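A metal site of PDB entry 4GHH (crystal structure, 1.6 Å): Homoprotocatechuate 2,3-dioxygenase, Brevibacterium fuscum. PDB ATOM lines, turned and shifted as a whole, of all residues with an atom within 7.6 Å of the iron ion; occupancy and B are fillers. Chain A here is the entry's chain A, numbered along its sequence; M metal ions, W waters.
The side-chain carboxylate (OE2) of Glu 267 is in hydrogen-bond range of the side-chain hydroxyl (OH) of Tyr 257, at 3.3 Å. OE2 of Glu 267 is in hydrogen-bond range of NE2 of His 248. The backbone NH (N) of Glu 267 sits at hydrogen-bond distance from the backbone carbonyl oxygen (O) of Val 215 (2.9 Å). N of Asn 157 sits at hydrogen-bond distance from O of His 214, 3.0 Å away. ND1 of His 214 is in hydrogen-bond range of ND1 of His 213 (2.8 Å). A ring nitrogen (NE2) of His 200 sits close to a ring nitrogen (ND1) of His 155 (3.3 Å). The backbone carbonyl oxygen (O) of His 155 lies within hydrogen-bond range of the backbone NH (N) of Ala 216 (2.9 Å). A ring nitrogen (ND1) of His 155 is in hydrogen-bond range of the side-chain carboxylate (OD2) of Asp 154 (2.7 Å).
His 200 touches the iron ion. Four residues have an atom within 4 Å of the iron ion: His 155, His 200, His 214 and Glu 267.
The iron ion is bound by OE1 of Glu 267, water W1, NE2 of His 214, NE2 of His 155, water W3 and water W2. The iron ion has six donor atoms within binding distance.
Water W2 bridges NE2 of His 200 and ND2 of Asn 157. Water W1 lies within hydrogen-bond range of OE2 of Glu 267 and NE2 of His 200.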
ATOM      1  N   ASP A 154      -1.388  36.694 -21.708  1.00  0.00           N
ATOM      2  CA  ASP A 154      -0.501  35.591 -22.059  1.00  0.00           C
ATOM      3  C   ASP A 154      -0.376  35.303 -23.559  1.00  0.00           C
ATOM      4  O   ASP A 154       0.750  35.106 -24.037  1.00  0.00           O
ATOM      5  CB  ASP A 154      -0.859  34.278 -21.344  1.00  0.00           C
ATOM      6  CG  ASP A 154       0.221  33.220 -21.567  1.00  0.00           C
ATOM      7  OD1 ASP A 154       1.299  33.357 -20.942  1.00  0.00           O
ATOM      8  OD2 ASP A 154       0.006  32.276 -22.370  1.00  0.00           O
ATOM      9  N   HIS A 155      -1.496  35.224 -24.266  1.00  0.00           N
ATOM     10  CA  HIS A 155      -1.464  34.876 -25.707  1.00  0.00           C
ATOM     11  C   HIS A 155      -2.721  35.172 -26.442  1.00  0.00           C
ATOM     12  O   HIS A 155      -3.751  35.472 -25.867  1.00  0.00           O
ATOM     13  CB  HIS A 155      -1.117  33.366 -25.894  1.00  0.00           C
ATOM     14  CG  HIS A 155      -2.168  32.422 -25.334  1.00  0.00           C
ATOM     15  ND1 HIS A 155      -2.109  31.922 -24.070  1.00  0.00           N
ATOM     16  CD2 HIS A 155      -3.324  31.896 -25.915  1.00  0.00           C
ATOM     17  CE1 HIS A 155      -3.161  31.100 -23.884  1.00  0.00           C
ATOM     18  NE2 HIS A 155      -3.898  31.084 -25.003  1.00  0.00           N
ATOM     19  N   PHE A 156      -2.620  35.054 -27.771  1.00  0.00           N
ATOM     20  CA  PHE A 156      -3.738  35.026 -28.664  1.00  0.00           C
ATOM     21  C   PHE A 156      -3.821  33.612 -29.284  1.00  0.00           C
ATOM     22  O   PHE A 156      -2.856  32.845 -29.290  1.00  0.00           O
ATOM     23  CB  PHE A 156      -3.497  36.013 -29.827  1.00  0.00           C
ATOM     24  CG  PHE A 156      -3.050  37.420 -29.406  1.00  0.00           C
ATOM     25  CD1 PHE A 156      -3.785  38.187 -28.503  1.00  0.00           C
ATOM     26  CD2 PHE A 156      -1.878  37.965 -29.935  1.00  0.00           C
ATOM     27  CE1 PHE A 156      -3.372  39.469 -28.181  1.00  0.00           C
ATOM     28  CE2 PHE A 156      -1.445  39.236 -29.601  1.00  0.00           C
ATOM     29  CZ  PHE A 156      -2.199  39.987 -28.727  1.00  0.00           C
ATOM     30  N   ASN A 157      -4.977  33.308 -29.834  1.00  0.00           N
ATOM     31  CA  ASN A 157      -5.182  32.096 -30.649  1.00  0.00           C
ATOM     32  C   ASN A 157      -6.041  32.454 -31.861  1.00  0.00           C
ATOM     33  O   ASN A 157      -7.134  32.980 -31.734  1.00  0.00           O
ATOM     34  CB  ASN A 157      -5.812  31.019 -29.794  1.00  0.00           C
ATOM     35  CG  ASN A 157      -5.904  29.685 -30.486  1.00  0.00           C
ATOM     36  OD1 ASN A 157      -6.542  29.559 -31.529  1.00  0.00           O
ATOM     37  ND2 ASN A 157      -5.296  28.662 -29.890  1.00  0.00           N
ATOM     38  N   TRP A 192       1.273  25.766 -31.587  1.00  0.00           N
ATOM     39  CA  TRP A 192       1.532  26.814 -30.603  1.00  0.00           C
ATOM     40  C   TRP A 192       2.934  27.329 -30.777  1.00  0.00           C
ATOM     41  O   TRP A 192       3.847  26.548 -30.953  1.00  0.00           O
ATOM     42  CB  TRP A 192       1.397  26.190 -29.219  1.00  0.00           C
ATOM     43  CG  TRP A 192      -0.035  25.903 -28.780  1.00  0.00           C
ATOM     44  CD1 TRP A 192      -0.776  26.620 -27.849  1.00  0.00           C
ATOM     45  CD2 TRP A 192      -0.884  24.823 -29.193  1.00  0.00           C
ATOM     46  NE1 TRP A 192      -2.017  26.095 -27.703  1.00  0.00           N
ATOM     47  CE2 TRP A 192      -2.155  25.006 -28.472  1.00  0.00           C
ATOM     48  CE3 TRP A 192      -0.754  23.748 -30.062  1.00  0.00           C
ATOM     49  CZ2 TRP A 192      -3.225  24.128 -28.630  1.00  0.00           C
ATOM     50  CZ3 TRP A 192      -1.836  22.892 -30.233  1.00  0.00           C
ATOM     51  CH2 TRP A 192      -3.038  23.065 -29.515  1.00  0.00           C
ATOM     52  N   HIS A 200       3.339  29.861 -25.519  1.00  0.00           N
ATOM     53  CA  HIS A 200       2.990  30.669 -26.689  1.00  0.00           C
ATOM     54  C   HIS A 200       2.751  32.142 -26.462  1.00  0.00           C
ATOM     55  O   HIS A 200       2.421  32.559 -25.356  1.00  0.00           O
ATOM     56  CB  HIS A 200       1.828  30.062 -27.477  1.00  0.00           C
ATOM     57  CG  HIS A 200       0.560  29.791 -26.697  1.00  0.00           C
ATOM     58  ND1 HIS A 200       0.547  29.287 -25.420  1.00  0.00           N
ATOM     59  CD2 HIS A 200      -0.766  29.834 -27.115  1.00  0.00           C
ATOM     60  CE1 HIS A 200      -0.769  29.060 -25.063  1.00  0.00           C
ATOM     61  NE2 HIS A 200      -1.535  29.365 -26.105  1.00  0.00           N
ATOM     62  N   ALA A 203      -1.056  31.227 -31.383  1.00  0.00           N
ATOM     63  CA  ALA A 203      -1.316  29.857 -31.722  1.00  0.00           C
ATOM     64  C   ALA A 203      -2.248  29.830 -32.903  1.00  0.00           C
ATOM     65  O   ALA A 203      -2.958  30.805 -33.181  1.00  0.00           O
ATOM     66  CB  ALA A 203      -1.939  29.119 -30.530  1.00  0.00           C
ATOM     67  N   THR A 205      -5.221  27.529 -34.757  1.00  0.00           N
ATOM     68  CA  THR A 205      -6.206  26.475 -34.685  1.00  0.00           C
ATOM     69  C   THR A 205      -6.787  26.305 -36.074  1.00  0.00           C
ATOM     70  O   THR A 205      -7.185  27.285 -36.706  1.00  0.00           O
ATOM     71  CB  THR A 205      -7.336  26.824 -33.684  1.00  0.00           C
ATOM     72  OG1 THR A 205      -6.764  27.048 -32.383  1.00  0.00           O
ATOM     73  CG2 THR A 205      -8.391  25.726 -33.642  1.00  0.00           C
ATOM     74  N   HIS A 213      -9.806  33.108 -32.267  1.00  0.00           N
ATOM     75  CA  HIS A 213     -10.394  32.143 -31.378  1.00  0.00           C
ATOM     76  C   HIS A 213     -10.549  32.705 -29.979  1.00  0.00           C
ATOM     77  O   HIS A 213     -11.650  32.639 -29.405  1.00  0.00           O
ATOM     78  CB  HIS A 213      -9.592  30.859 -31.377  1.00  0.00           C
ATOM     79  CG  HIS A 213     -10.367  29.721 -30.802  1.00  0.00           C
ATOM     80  ND1 HIS A 213     -10.522  29.547 -29.467  1.00  0.00           N
ATOM     81  CD2 HIS A 213     -11.149  28.749 -31.423  1.00  0.00           C
ATOM     82  CE1 HIS A 213     -11.316  28.484 -29.256  1.00  0.00           C
ATOM     83  NE2 HIS A 213     -11.701  27.998 -30.453  1.00  0.00           N
ATOM     84  N   HIS A 214      -9.472  33.221 -29.405  1.00  0.00           N
ATOM     85  CA  HIS A 214      -9.535  33.844 -28.065  1.00  0.00           C
ATOM     86  C   HIS A 214      -8.330  34.696 -27.776  1.00  0.00           C
ATOM     87  O   HIS A 214      -7.304  34.612 -28.455  1.00  0.00           O
ATOM     88  CB  HIS A 214      -9.725  32.767 -26.968  1.00  0.00           C
ATOM     89  CG  HIS A 214      -8.604  31.711 -26.905  1.00  0.00           C
ATOM     90  ND1 HIS A 214      -8.657  30.547 -27.583  1.00  0.00           N
ATOM     91  CD2 HIS A 214      -7.419  31.671 -26.151  1.00  0.00           C
ATOM     92  CE1 HIS A 214      -7.576  29.794 -27.303  1.00  0.00           C
ATOM     93  NE2 HIS A 214      -6.802  30.476 -26.427  1.00  0.00           N
ATOM     94  N   VAL A 215      -8.468  35.493 -26.694  1.00  0.00           N
ATOM     95  CA  VAL A 215      -7.381  36.179 -26.046  1.00  0.00           C
ATOM     96  C   VAL A 215      -7.277  35.552 -24.637  1.00  0.00           C
ATOM     97  O   VAL A 215      -8.300  35.276 -24.017  1.00  0.00           O
ATOM     98  CB  VAL A 215      -7.703  37.690 -25.929  1.00  0.00           C
ATOM     99  CG1 VAL A 215      -6.606  38.409 -25.166  1.00  0.00           C
ATOM    100  CG2 VAL A 215      -7.874  38.275 -27.336  1.00  0.00           C
ATOM    101  N   ALA A 216      -6.060  35.341 -24.161  1.00  0.00           N
ATOM    102  CA  ALA A 216      -5.858  34.661 -22.891  1.00  0.00           C
ATOM    103  C   ALA A 216      -5.122  35.558 -21.897  1.00  0.00           C
ATOM    104  O   ALA A 216      -4.090  36.165 -22.228  1.00  0.00           O
ATOM    105  CB  ALA A 216      -5.070  33.360 -23.104  1.00  0.00           C
ATOM    106  N   HIS A 248      -5.045  21.601 -19.338  1.00  0.00           N
ATOM    107  CA  HIS A 248      -4.689  21.285 -20.723  1.00  0.00           C
ATOM    108  C   HIS A 248      -3.682  20.166 -20.795  1.00  0.00           C
ATOM    109  O   HIS A 248      -2.800  20.037 -19.915  1.00  0.00           O
ATOM    110  CB  HIS A 248      -4.069  22.496 -21.421  1.00  0.00           C
ATOM    111  CG  HIS A 248      -5.042  23.542 -21.835  1.00  0.00           C
ATOM    112  ND1 HIS A 248      -6.180  23.264 -22.550  1.00  0.00           N
ATOM    113  CD2 HIS A 248      -4.993  24.944 -21.691  1.00  0.00           C
ATOM    114  CE1 HIS A 248      -6.798  24.429 -22.861  1.00  0.00           C
ATOM    115  NE2 HIS A 248      -6.098  25.446 -22.292  1.00  0.00           N
ATOM    116  N   SER A 251       0.394  22.394 -23.535  1.00  0.00           N
ATOM    117  CA  SER A 251       0.707  23.525 -22.631  1.00  0.00           C
ATOM    118  C   SER A 251       0.788  23.207 -21.138  1.00  0.00           C
ATOM    119  O   SER A 251       1.457  23.927 -20.417  1.00  0.00           O
ATOM    120  CB  SER A 251      -0.181  24.755 -22.826  1.00  0.00           C
ATOM    121  OG  SER A 251      -1.403  24.682 -22.100  1.00  0.00           O
ATOM    122  N   TYR A 255      -6.885  26.021 -16.986  1.00  0.00           N
ATOM    123  CA  TYR A 255      -7.603  26.896 -17.908  1.00  0.00           C
ATOM    124  C   TYR A 255      -9.099  26.982 -17.683  1.00  0.00           C
ATOM    125  O   TYR A 255      -9.702  26.165 -16.962  1.00  0.00           O
ATOM    126  CB  TYR A 255      -7.342  26.423 -19.343  1.00  0.00           C
ATOM    127  CG  TYR A 255      -8.160  25.178 -19.713  1.00  0.00           C
ATOM    128  CD1 TYR A 255      -7.599  23.908 -19.586  1.00  0.00           C
ATOM    129  CD2 TYR A 255      -9.457  25.287 -20.201  1.00  0.00           C
ATOM    130  CE1 TYR A 255      -8.353  22.767 -19.878  1.00  0.00           C
ATOM    131  CE2 TYR A 255     -10.199  24.158 -20.531  1.00  0.00           C
ATOM    132  CZ  TYR A 255      -9.635  22.900 -20.369  1.00  0.00           C
ATOM    133  OH  TYR A 255     -10.380  21.763 -20.711  1.00  0.00           O
ATOM    134  N   TYR A 257     -12.502  28.809 -20.258  1.00  0.00           N
ATOM    135  CA  TYR A 257     -12.987  29.639 -21.388  1.00  0.00           C
ATOM    136  C   TYR A 257     -14.364  30.216 -21.060  1.00  0.00           C
ATOM    137  O   TYR A 257     -15.323  29.478 -20.746  1.00  0.00           O
ATOM    138  CB  TYR A 257     -13.116  28.831 -22.688  1.00  0.00           C
ATOM    139  CG  TYR A 257     -11.793  28.253 -23.159  1.00  0.00           C
ATOM    140  CD1 TYR A 257     -10.890  28.997 -23.911  1.00  0.00           C
ATOM    141  CD2 TYR A 257     -11.441  26.953 -22.840  1.00  0.00           C
ATOM    142  CE1 TYR A 257      -9.679  28.471 -24.326  1.00  0.00           C
ATOM    143  CE2 TYR A 257     -10.229  26.423 -23.280  1.00  0.00           C
ATOM    144  CZ  TYR A 257      -9.351  27.177 -24.005  1.00  0.00           C
ATOM    145  OH  TYR A 257      -8.187  26.628 -24.436  1.00  0.00           O
ATOM    146  N   GLU A 267      -9.836  33.276 -22.524  1.00  0.00           N
ATOM    147  CA  GLU A 267      -9.292  32.187 -21.760  1.00  0.00           C
ATOM    148  C   GLU A 267      -8.614  32.766 -20.512  1.00  0.00           C
ATOM    149  O   GLU A 267      -7.926  33.777 -20.589  1.00  0.00           O
ATOM    150  CB  GLU A 267      -8.235  31.417 -22.555  1.00  0.00           C
ATOM    151  CG  GLU A 267      -7.810  30.128 -21.849  1.00  0.00           C
ATOM    152  CD  GLU A 267      -6.750  29.359 -22.610  1.00  0.00           C
ATOM    153  OE1 GLU A 267      -6.273  29.877 -23.609  1.00  0.00           O
ATOM    154  OE2 GLU A 267      -6.410  28.226 -22.218  1.00  0.00           O
ATOM    155  N   ILE A 268      -8.791  32.079 -19.381  1.00  0.00           N
ATOM    156  CA  ILE A 268      -7.995  32.340 -18.210  1.00  0.00           C
ATOM    157  C   ILE A 268      -7.048  31.125 -18.076  1.00  0.00           C
ATOM    158  O   ILE A 268      -7.502  29.993 -18.201  1.00  0.00           O
ATOM    159  CB  ILE A 268      -8.839  32.525 -16.954  1.00  0.00           C
ATOM    160  CG1 ILE A 268     -10.139  33.321 -17.239  1.00  0.00           C
ATOM    161  CG2 ILE A 268      -8.008  33.166 -15.853  1.00  0.00           C
ATOM    162  CD1 ILE A 268      -9.907  34.739 -17.675  1.00  0.00           C
ATOM    163  N   TYR A 269      -5.787  31.375 -17.774  1.00  0.00           N
ATOM    164  CA  TYR A 269      -4.703  30.418 -17.979  1.00  0.00           C
ATOM    165  C   TYR A 269      -3.642  30.545 -16.902  1.00  0.00           C
ATOM    166  O   TYR A 269      -3.332  31.669 -16.478  1.00  0.00           O
ATOM    167  CB  TYR A 269      -4.102  30.799 -19.331  1.00  0.00           C
ATOM    168  CG  TYR A 269      -3.006  29.999 -19.958  1.00  0.00           C
ATOM    169  CD1 TYR A 269      -3.277  28.998 -20.892  1.00  0.00           C
ATOM    170  CD2 TYR A 269      -1.674  30.346 -19.741  1.00  0.00           C
ATOM    171  CE1 TYR A 269      -2.239  28.332 -21.542  1.00  0.00           C
ATOM    172  CE2 TYR A 269      -0.630  29.669 -20.385  1.00  0.00           C
ATOM    173  CZ  TYR A 269      -0.919  28.657 -21.289  1.00  0.00           C
ATOM    174  OH  TYR A 269       0.116  28.016 -21.956  1.00  0.00           O
ATOM    175  N   ARG A 293      -6.352  18.006 -25.138  1.00  0.00           N
ATOM    176  CA  ARG A 293      -6.922  19.325 -24.909  1.00  0.00           C
ATOM    177  C   ARG A 293      -7.353  19.526 -23.485  1.00  0.00           C
ATOM    178  O   ARG A 293      -7.045  20.524 -22.867  1.00  0.00           O
ATOM    179  CB  ARG A 293      -8.070  19.635 -25.868  1.00  0.00           C
ATOM    180  CG  ARG A 293      -7.587  19.838 -27.285  1.00  0.00           C
ATOM    181  CD  ARG A 293      -8.536  20.639 -28.136  1.00  0.00           C
ATOM    182  NE  ARG A 293      -7.958  20.982 -29.438  1.00  0.00           N
ATOM    183  CZ  ARG A 293      -7.237  22.061 -29.747  1.00  0.00           C
ATOM    184  NH1 ARG A 293      -6.910  22.959 -28.827  1.00  0.00           N
ATOM    185  NH2 ARG A 293      -6.815  22.254 -31.009  1.00  0.00           N
ATOM    186  N   TRP A 304     -16.750  25.200 -29.082  1.00  0.00           N
ATOM    187  CA  TRP A 304     -15.346  25.595 -28.926  1.00  0.00           C
ATOM    188  C   TRP A 304     -14.630  25.472 -30.253  1.00  0.00           C
ATOM    189  O   TRP A 304     -13.703  26.248 -30.565  1.00  0.00           O
ATOM    190  CB  TRP A 304     -14.695  24.770 -27.801  1.00  0.00           C
ATOM    191  CG  TRP A 304     -13.379  25.346 -27.360  1.00  0.00           C
ATOM    192  CD1 TRP A 304     -13.169  26.286 -26.350  1.00  0.00           C
ATOM    193  CD2 TRP A 304     -12.077  25.072 -27.921  1.00  0.00           C
ATOM    194  NE1 TRP A 304     -11.853  26.617 -26.276  1.00  0.00           N
ATOM    195  CE2 TRP A 304     -11.141  25.917 -27.211  1.00  0.00           C
ATOM    196  CE3 TRP A 304     -11.607  24.283 -28.966  1.00  0.00           C
ATOM    197  CZ2 TRP A 304      -9.791  25.923 -27.502  1.00  0.00           C
ATOM    198  CZ3 TRP A 304     -10.250  24.300 -29.260  1.00  0.00           C
ATOM    199  CH2 TRP A 304      -9.354  25.105 -28.536  1.00  0.00           C
HETATM  200 FE    FE M   1      -5.255  29.422 -25.361  1.00  0.00          FE
HETATM  201  O   HOH W   1      -4.011  28.029 -24.365  1.00  0.00           O
HETATM  202  O   HOH W   2      -4.019  28.973 -27.325  1.00  0.00           O
HETATM  203  O   HOH W   3      -6.319  27.519 -25.790  1.00  0.00           O
